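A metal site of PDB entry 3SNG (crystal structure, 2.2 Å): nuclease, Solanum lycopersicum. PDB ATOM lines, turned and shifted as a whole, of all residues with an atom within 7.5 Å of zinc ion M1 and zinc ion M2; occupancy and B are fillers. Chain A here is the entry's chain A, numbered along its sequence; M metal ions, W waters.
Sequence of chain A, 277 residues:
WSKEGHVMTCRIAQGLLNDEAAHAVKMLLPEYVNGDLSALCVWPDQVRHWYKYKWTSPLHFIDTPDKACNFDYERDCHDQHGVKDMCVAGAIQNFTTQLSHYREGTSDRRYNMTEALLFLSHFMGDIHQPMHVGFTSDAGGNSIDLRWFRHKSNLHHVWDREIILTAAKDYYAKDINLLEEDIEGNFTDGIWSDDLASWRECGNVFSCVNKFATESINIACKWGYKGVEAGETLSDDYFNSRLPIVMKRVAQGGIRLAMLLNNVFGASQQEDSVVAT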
ATOM      1  N   TRP A   1       7.115   2.322  -4.343  1.00  0.00           N
ATOM      2  CA  TRP A   1       8.391   2.655  -4.975  1.00  0.00           C
ATOM      3  C   TRP A   1       9.155   1.392  -5.359  1.00  0.00           C
ATOM      4  O   TRP A   1       8.924   0.305  -4.795  1.00  0.00           O
ATOM      5  CB  TRP A   1       9.292   3.423  -4.014  1.00  0.00           C
ATOM      6  CG  TRP A   1       8.731   4.633  -3.401  1.00  0.00           C
ATOM      7  CD1 TRP A   1       8.331   4.765  -2.142  1.00  0.00           C
ATOM      8  CD2 TRP A   1       8.588   5.936  -4.008  1.00  0.00           C
ATOM      9  NE1 TRP A   1       7.908   6.035  -1.901  1.00  0.00           N
ATOM     10  CE2 TRP A   1       8.056   6.787  -3.040  1.00  0.00           C
ATOM     11  CE3 TRP A   1       8.844   6.452  -5.278  1.00  0.00           C
ATOM     12  CZ2 TRP A   1       7.770   8.129  -3.275  1.00  0.00           C
ATOM     13  CZ3 TRP A   1       8.566   7.794  -5.528  1.00  0.00           C
ATOM     14  CH2 TRP A   1       8.028   8.611  -4.529  1.00  0.00           C
ATOM     15  N   SER A   2      10.072   1.559  -6.288  1.00  0.00           N
ATOM     16  CA  SER A   2      11.135   0.559  -6.504  1.00  0.00           C
ATOM     17  C   SER A   2      12.217   0.803  -5.454  1.00  0.00           C
ATOM     18  O   SER A   2      12.038   1.593  -4.511  1.00  0.00           O
ATOM     19  CB  SER A   2      11.710   0.682  -7.906  1.00  0.00           C
ATOM     20  OG  SER A   2      10.689   0.537  -8.865  1.00  0.00           O
ATOM     21  N   LYS A   3      13.339   0.121  -5.609  1.00  0.00           N
ATOM     22  CA  LYS A   3      14.346   0.037  -4.564  1.00  0.00           C
ATOM     23  C   LYS A   3      14.814   1.387  -4.054  1.00  0.00           C
ATOM     24  O   LYS A   3      14.845   1.615  -2.827  1.00  0.00           O
ATOM     25  CB  LYS A   3      15.520  -0.827  -5.079  1.00  0.00           C
ATOM     26  CG  LYS A   3      16.795  -0.729  -4.276  1.00  0.00           C
ATOM     27  CD  LYS A   3      17.964  -1.486  -4.951  1.00  0.00           C
ATOM     28  CE  LYS A   3      18.625  -0.653  -6.062  1.00  0.00           C
ATOM     29  NZ  LYS A   3      19.949  -1.210  -6.482  1.00  0.00           N
ATOM     30  N   GLY A   5      13.470   4.488  -3.951  1.00  0.00           N
ATOM     31  CA  GLY A   5      12.548   5.270  -3.092  1.00  0.00           C
ATOM     32  C   GLY A   5      12.439   4.710  -1.679  1.00  0.00           C
ATOM     33  O   GLY A   5      12.363   5.447  -0.716  1.00  0.00           O
ATOM     34  N   HIS A   6      12.393   3.381  -1.574  1.00  0.00           N
ATOM     35  CA  HIS A   6      12.336   2.709  -0.266  1.00  0.00           C
ATOM     36  C   HIS A   6      13.600   2.914   0.540  1.00  0.00           C
ATOM     37  O   HIS A   6      13.549   3.212   1.756  1.00  0.00           O
ATOM     38  CB  HIS A   6      12.031   1.222  -0.480  1.00  0.00           C
ATOM     39  CG  HIS A   6      10.596   0.987  -0.854  1.00  0.00           C
ATOM     40  ND1 HIS A   6       9.561   1.321  -0.021  1.00  0.00           N
ATOM     41  CD2 HIS A   6      10.034   0.467  -1.968  1.00  0.00           C
ATOM     42  CE1 HIS A   6       8.416   1.025  -0.604  1.00  0.00           C
ATOM     43  NE2 HIS A   6       8.666   0.534  -1.800  1.00  0.00           N
ATOM     44  N   CYS A  41      14.474  -2.695   3.431  1.00  0.00           N
ATOM     45  CA  CYS A  41      13.171  -2.063   3.198  1.00  0.00           C
ATOM     46  C   CYS A  41      12.541  -2.507   1.881  1.00  0.00           C
ATOM     47  O   CYS A  41      11.336  -2.321   1.667  1.00  0.00           O
ATOM     48  CB  CYS A  41      13.274  -0.535   3.286  1.00  0.00           C
ATOM     49  SG  CYS A  41      14.347   0.114   2.056  1.00  0.00           S
ATOM     50  N   VAL A  42      13.346  -3.129   1.030  1.00  0.00           N
ATOM     51  CA  VAL A  42      12.860  -3.707  -0.186  1.00  0.00           C
ATOM     52  C   VAL A  42      12.287  -5.090   0.044  1.00  0.00           C
ATOM     53  O   VAL A  42      11.580  -5.601  -0.807  1.00  0.00           O
ATOM     54  CB  VAL A  42      13.976  -3.776  -1.272  1.00  0.00           C
ATOM     55  CG1 VAL A  42      13.435  -4.302  -2.569  1.00  0.00           C
ATOM     56  CG2 VAL A  42      14.504  -2.385  -1.524  1.00  0.00           C
ATOM     57  N   PRO A  44       9.791  -6.532   1.442  1.00  0.00           N
ATOM     58  CA  PRO A  44       8.429  -6.896   1.057  1.00  0.00           C
ATOM     59  C   PRO A  44       8.174  -7.035  -0.462  1.00  0.00           C
ATOM     60  O   PRO A  44       7.319  -7.809  -0.874  1.00  0.00           O
ATOM     61  CB  PRO A  44       7.598  -5.778   1.658  1.00  0.00           C
ATOM     62  CG  PRO A  44       8.361  -5.373   2.861  1.00  0.00           C
ATOM     63  CD  PRO A  44       9.799  -5.423   2.399  1.00  0.00           C
ATOM     64  N   ASP A  45       8.893  -6.303  -1.303  1.00  0.00           N
ATOM     65  CA  ASP A  45       8.809  -6.482  -2.737  1.00  0.00           C
ATOM     66  C   ASP A  45       9.407  -7.815  -3.250  1.00  0.00           C
ATOM     67  O   ASP A  45       9.073  -8.290  -4.346  1.00  0.00           O
ATOM     68  CB  ASP A  45       9.418  -5.267  -3.470  1.00  0.00           C
ATOM     69  CG  ASP A  45       8.420  -4.073  -3.557  1.00  0.00           C
ATOM     70  OD1 ASP A  45       7.209  -4.301  -3.263  1.00  0.00           O
ATOM     71  OD2 ASP A  45       8.823  -2.945  -3.911  1.00  0.00           O
ATOM     72  N   ARG A  48       6.651 -10.657  -1.746  1.00  0.00           N
ATOM     73  CA  ARG A  48       5.280 -10.653  -2.246  1.00  0.00           C
ATOM     74  C   ARG A  48       5.024 -11.725  -3.325  1.00  0.00           C
ATOM     75  O   ARG A  48       3.890 -12.126  -3.566  1.00  0.00           O
ATOM     76  CB  ARG A  48       4.894  -9.299  -2.818  1.00  0.00           C
ATOM     77  CG  ARG A  48       5.594  -8.940  -4.091  1.00  0.00           C
ATOM     78  CD  ARG A  48       5.428  -7.491  -4.465  1.00  0.00           C
ATOM     79  NE  ARG A  48       4.073  -7.142  -4.860  1.00  0.00           N
ATOM     80  CZ  ARG A  48       3.678  -5.903  -5.182  1.00  0.00           C
ATOM     81  NH1 ARG A  48       4.547  -4.899  -5.177  1.00  0.00           N
ATOM     82  NH2 ARG A  48       2.419  -5.663  -5.546  1.00  0.00           N
ATOM     83  N   THR A  56       0.179 -10.840   1.031  1.00  0.00           N
ATOM     84  CA  THR A  56       0.755  -9.477   1.066  1.00  0.00           C
ATOM     85  C   THR A  56       0.617  -8.664  -0.200  1.00  0.00           C
ATOM     86  O   THR A  56       0.866  -7.448  -0.183  1.00  0.00           O
ATOM     87  CB  THR A  56       2.257  -9.465   1.423  1.00  0.00           C
ATOM     88  OG1 THR A  56       3.053  -9.974   0.320  1.00  0.00           O
ATOM     89  CG2 THR A  56       2.504 -10.268   2.685  1.00  0.00           C
ATOM     90  N   SER A  57       0.285  -9.310  -1.307  1.00  0.00           N
ATOM     91  CA  SER A  57       0.274  -8.629  -2.591  1.00  0.00           C
ATOM     92  C   SER A  57      -0.690  -7.421  -2.630  1.00  0.00           C
ATOM     93  O   SER A  57      -0.285  -6.338  -3.014  1.00  0.00           O
ATOM     94  CB  SER A  57      -0.077  -9.591  -3.702  1.00  0.00           C
ATOM     95  OG  SER A  57      -0.386  -8.864  -4.862  1.00  0.00           O
ATOM     96  N   LEU A  59      -1.460  -5.580  -0.312  1.00  0.00           N
ATOM     97  CA  LEU A  59      -1.135  -4.607   0.708  1.00  0.00           C
ATOM     98  C   LEU A  59      -0.188  -3.486   0.240  1.00  0.00           C
ATOM     99  O   LEU A  59       0.116  -2.570   1.027  1.00  0.00           O
ATOM    100  CB  LEU A  59      -0.508  -5.273   1.893  1.00  0.00           C
ATOM    101  CG  LEU A  59      -1.308  -6.359   2.528  1.00  0.00           C
ATOM    102  CD1 LEU A  59      -0.621  -6.848   3.792  1.00  0.00           C
ATOM    103  CD2 LEU A  59      -2.764  -5.842   2.796  1.00  0.00           C
ATOM    104  N   HIS A  60       0.313  -3.556  -0.991  1.00  0.00           N
ATOM    105  CA  HIS A  60       1.241  -2.509  -1.473  1.00  0.00           C
ATOM    106  C   HIS A  60       0.576  -1.254  -2.062  1.00  0.00           C
ATOM    107  O   HIS A  60       1.268  -0.234  -2.342  1.00  0.00           O
ATOM    108  CB  HIS A  60       2.191  -3.091  -2.524  1.00  0.00           C
ATOM    109  CG  HIS A  60       3.160  -4.077  -1.977  1.00  0.00           C
ATOM    110  ND1 HIS A  60       4.503  -3.799  -1.823  1.00  0.00           N
ATOM    111  CD2 HIS A  60       2.965  -5.317  -1.492  1.00  0.00           C
ATOM    112  CE1 HIS A  60       5.095  -4.851  -1.290  1.00  0.00           C
ATOM    113  NE2 HIS A  60       4.178  -5.791  -1.070  1.00  0.00           N
ATOM    114  N   PHE A  61      -0.742  -1.292  -2.264  1.00  0.00           N
ATOM    115  CA  PHE A  61      -1.407  -0.245  -3.031  1.00  0.00           C
ATOM    116  C   PHE A  61      -2.859  -0.072  -2.613  1.00  0.00           C
ATOM    117  O   PHE A  61      -3.347  -0.759  -1.745  1.00  0.00           O
ATOM    118  CB  PHE A  61      -1.331  -0.544  -4.537  1.00  0.00           C
ATOM    119  CG  PHE A  61      -1.955  -1.864  -4.932  1.00  0.00           C
ATOM    120  CD1 PHE A  61      -3.318  -1.963  -5.135  1.00  0.00           C
ATOM    121  CD2 PHE A  61      -1.181  -2.981  -5.111  1.00  0.00           C
ATOM    122  CE1 PHE A  61      -3.905  -3.165  -5.439  1.00  0.00           C
ATOM    123  CE2 PHE A  61      -1.769  -4.200  -5.447  1.00  0.00           C
ATOM    124  CZ  PHE A  61      -3.136  -4.283  -5.627  1.00  0.00           C
ATOM    125  N   VAL A  88      -2.830  -0.887   1.356  1.00  0.00           N
ATOM    126  CA  VAL A  88      -1.636  -0.323   2.024  1.00  0.00           C
ATOM    127  C   VAL A  88      -2.036   0.485   3.270  1.00  0.00           C
ATOM    128  O   VAL A  88      -1.345   0.412   4.303  1.00  0.00           O
ATOM    129  CB  VAL A  88      -0.737   0.444   1.045  1.00  0.00           C
ATOM    130  CG1 VAL A  88      -1.396   1.755   0.617  1.00  0.00           C
ATOM    131  CG2 VAL A  88       0.671   0.696   1.662  1.00  0.00           C
ATOM    132  N   HIS A 122       8.288  -0.380   4.660  1.00  0.00           N
ATOM    133  CA  HIS A 122       8.043  -0.432   3.239  1.00  0.00           C
ATOM    134  C   HIS A 122       6.694   0.206   2.880  1.00  0.00           C
ATOM    135  O   HIS A 122       6.603   1.010   1.957  1.00  0.00           O
ATOM    136  CB  HIS A 122       8.064  -1.887   2.784  1.00  0.00           C
ATOM    137  CG  HIS A 122       7.891  -2.065   1.306  1.00  0.00           C
ATOM    138  ND1 HIS A 122       8.958  -2.177   0.448  1.00  0.00           N
ATOM    139  CD2 HIS A 122       6.773  -2.152   0.541  1.00  0.00           C
ATOM    140  CE1 HIS A 122       8.509  -2.304  -0.793  1.00  0.00           C
ATOM    141  NE2 HIS A 122       7.184  -2.281  -0.770  1.00  0.00           N
ATOM    142  N   PHE A 123       5.637  -0.172   3.582  1.00  0.00           N
ATOM    143  CA  PHE A 123       4.294   0.309   3.219  1.00  0.00           C
ATOM    144  C   PHE A 123       4.139   1.811   3.453  1.00  0.00           C
ATOM    145  O   PHE A 123       3.432   2.464   2.706  1.00  0.00           O
ATOM    146  CB  PHE A 123       3.210  -0.491   3.936  1.00  0.00           C
ATOM    147  CG  PHE A 123       3.132  -1.941   3.478  1.00  0.00           C
ATOM    148  CD1 PHE A 123       3.321  -2.278   2.157  1.00  0.00           C
ATOM    149  CD2 PHE A 123       2.893  -2.951   4.370  1.00  0.00           C
ATOM    150  CE1 PHE A 123       3.271  -3.618   1.714  1.00  0.00           C
ATOM    151  CE2 PHE A 123       2.828  -4.321   3.928  1.00  0.00           C
ATOM    152  CZ  PHE A 123       3.041  -4.625   2.623  1.00  0.00           C
ATOM    153  N   GLY A 125       6.365   3.871   2.762  1.00  0.00           N
ATOM    154  CA  GLY A 125       6.869   4.332   1.479  1.00  0.00           C
ATOM    155  C   GLY A 125       5.802   4.188   0.407  1.00  0.00           C
ATOM    156  O   GLY A 125       5.488   5.140  -0.276  1.00  0.00           O
ATOM    157  N   ASP A 126       5.216   3.001   0.283  1.00  0.00           N
ATOM    158  CA  ASP A 126       4.249   2.769  -0.762  1.00  0.00           C
ATOM    159  C   ASP A 126       3.049   3.741  -0.708  1.00  0.00           C
ATOM    160  O   ASP A 126       2.625   4.225  -1.748  1.00  0.00           O
ATOM    161  CB  ASP A 126       3.779   1.288  -0.794  1.00  0.00           C
ATOM    162  CG  ASP A 126       4.773   0.366  -1.534  1.00  0.00           C
ATOM    163  OD1 ASP A 126       5.679   0.885  -2.161  1.00  0.00           O
ATOM    164  OD2 ASP A 126       4.599  -0.867  -1.579  1.00  0.00           O
ATOM    165  N   ILE A 127       2.513   4.018   0.479  1.00  0.00           N
ATOM    166  CA  ILE A 127       1.321   4.843   0.549  1.00  0.00           C
ATOM    167  C   ILE A 127       1.617   6.271   0.074  1.00  0.00           C
ATOM    168  O   ILE A 127       0.728   6.947  -0.358  1.00  0.00           O
ATOM    169  CB  ILE A 127       0.712   4.881   1.947  1.00  0.00           C
ATOM    170  CG1 ILE A 127      -0.751   5.374   1.867  1.00  0.00           C
ATOM    171  CG2 ILE A 127       1.537   5.726   2.895  1.00  0.00           C
ATOM    172  CD1 ILE A 127      -1.556   5.127   3.148  1.00  0.00           C
ATOM    173  N   GLN A 129       3.784   6.907  -2.468  1.00  0.00           N
ATOM    174  CA  GLN A 129       4.012   6.891  -3.924  1.00  0.00           C
ATOM    175  C   GLN A 129       2.656   7.131  -4.592  1.00  0.00           C
ATOM    176  O   GLN A 129       1.764   6.280  -4.524  1.00  0.00           O
ATOM    177  CB  GLN A 129       4.588   5.539  -4.376  1.00  0.00           C
ATOM    178  CG  GLN A 129       5.501   5.597  -5.656  1.00  0.00           C
ATOM    179  CD  GLN A 129       4.738   5.805  -6.966  1.00  0.00           C
ATOM    180  OE1 GLN A 129       3.982   6.783  -7.088  1.00  0.00           O
ATOM    181  NE2 GLN A 129       4.910   4.884  -7.933  1.00  0.00           N
ATOM    182  N   HIS A 132       0.740   4.420  -6.371  1.00  0.00           N
ATOM    183  CA  HIS A 132       0.239   3.325  -5.520  1.00  0.00           C
ATOM    184  C   HIS A 132      -1.180   3.554  -4.979  1.00  0.00           C
ATOM    185  O   HIS A 132      -1.757   2.645  -4.364  1.00  0.00           O
ATOM    186  CB  HIS A 132       1.212   3.054  -4.362  1.00  0.00           C
ATOM    187  CG  HIS A 132       2.379   2.212  -4.772  1.00  0.00           C
ATOM    188  ND1 HIS A 132       2.621   0.977  -4.229  1.00  0.00           N
ATOM    189  CD2 HIS A 132       3.287   2.389  -5.744  1.00  0.00           C
ATOM    190  CE1 HIS A 132       3.682   0.437  -4.829  1.00  0.00           C
ATOM    191  NE2 HIS A 132       4.099   1.277  -5.737  1.00  0.00           N
ATOM    192  N   HIS A 156       3.176   3.897 -14.051  1.00  0.00           N
ATOM    193  CA  HIS A 156       3.515   3.478 -12.662  1.00  0.00           C
ATOM    194  C   HIS A 156       5.017   3.488 -12.408  1.00  0.00           C
ATOM    195  O   HIS A 156       5.509   4.056 -11.401  1.00  0.00           O
ATOM    196  CB  HIS A 156       2.946   2.120 -12.380  1.00  0.00           C
ATOM    197  CG  HIS A 156       3.020   1.716 -10.929  1.00  0.00           C
ATOM    198  ND1 HIS A 156       1.965   1.866 -10.060  1.00  0.00           N
ATOM    199  CD2 HIS A 156       4.021   1.139 -10.215  1.00  0.00           C
ATOM    200  CE1 HIS A 156       2.303   1.394  -8.870  1.00  0.00           C
ATOM    201  NE2 HIS A 156       3.546   0.960  -8.930  1.00  0.00           N
ATOM    202  N   ASP A 160       7.540   5.021  -9.731  1.00  0.00           N
ATOM    203  CA  ASP A 160       8.257   4.082  -8.846  1.00  0.00           C
ATOM    204  C   ASP A 160       9.763   4.247  -8.949  1.00  0.00           C
ATOM    205  O   ASP A 160      10.462   4.079  -7.953  1.00  0.00           O
ATOM    206  CB  ASP A 160       7.963   2.634  -9.197  1.00  0.00           C
ATOM    207  CG  ASP A 160       6.839   2.003  -8.377  1.00  0.00           C
ATOM    208  OD1 ASP A 160       6.247   2.593  -7.467  1.00  0.00           O
ATOM    209  OD2 ASP A 160       6.557   0.861  -8.651  1.00  0.00           O
HETATM  210 ZN    ZN M   1       5.796  -2.278  -2.260  1.00  0.00          ZN
HETATM  211 ZN    ZN M   2       7.354   0.427  -3.340  1.00  0.00          ZN
HETATM  212 ZN    ZN M   3       4.901   0.309  -7.469  1.00  0.00          ZN
HETATM  213  O   HOH W   1       6.602  -1.229  -3.675  1.00  0.00           O
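The indole nitrogen (NE1) of Trp 1 lies within hydrogen-bond range of the backbone carbonyl oxygen (O) of Gly 125 (3.0 Å). OD1 of Asp 45 sits close to ND1 of His 60 (3.1 Å). The side-chain carboxylate (OD1) of Asp 45 is in salt-bridge range of the guanidinium group (NH1) of Arg 48 (3.3 Å). ND1 of His 132 is in hydrogen-bond range of O of His 60. OD1 of Asp 160 lies close to N of Trp 1. NE2 of His 122 sits close to OD1 of Asp 45 (3.2 Å). O of Cys 41 lies within hydrogen-bond range of ND1 of His 122. The side-chain sulfur (SG) of Cys 41 lies within hydrogen-bond range of the backbone carbonyl oxygen (O) of His 6, 3.2 Å away.
Merely in contact with zinc ion M2: His 132 (3.96 Å). Within 4 Å of zinc ion M2: Trp 1, His 6, Asp 45, His 122, Asp 126 and His 132.
Zinc ion M1 is bound by water W1 (1.9 Å), OD2 of Asp 126 (2.0 Å), NE2 of His 122 (2.0 Å) and ND1 of His 60 (2.0 Å). Zinc ion M1 has four donor atoms within binding distance. Slightly farther from zinc ion M1 lies the side-chain carboxylate (OD1) of Asp 45 (2.7 Å).
Zinc ion M2 is bound by water W1 (1.8 Å), a ring nitrogen (NE2) of His 6 (2.0 Å), the side-chain carboxylate of Asp 126 (2.1 Å), the backbone carbonyl oxygen of Trp 1 (2.1 Å) and the backbone nitrogen of Trp 1 (2.2 Å).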
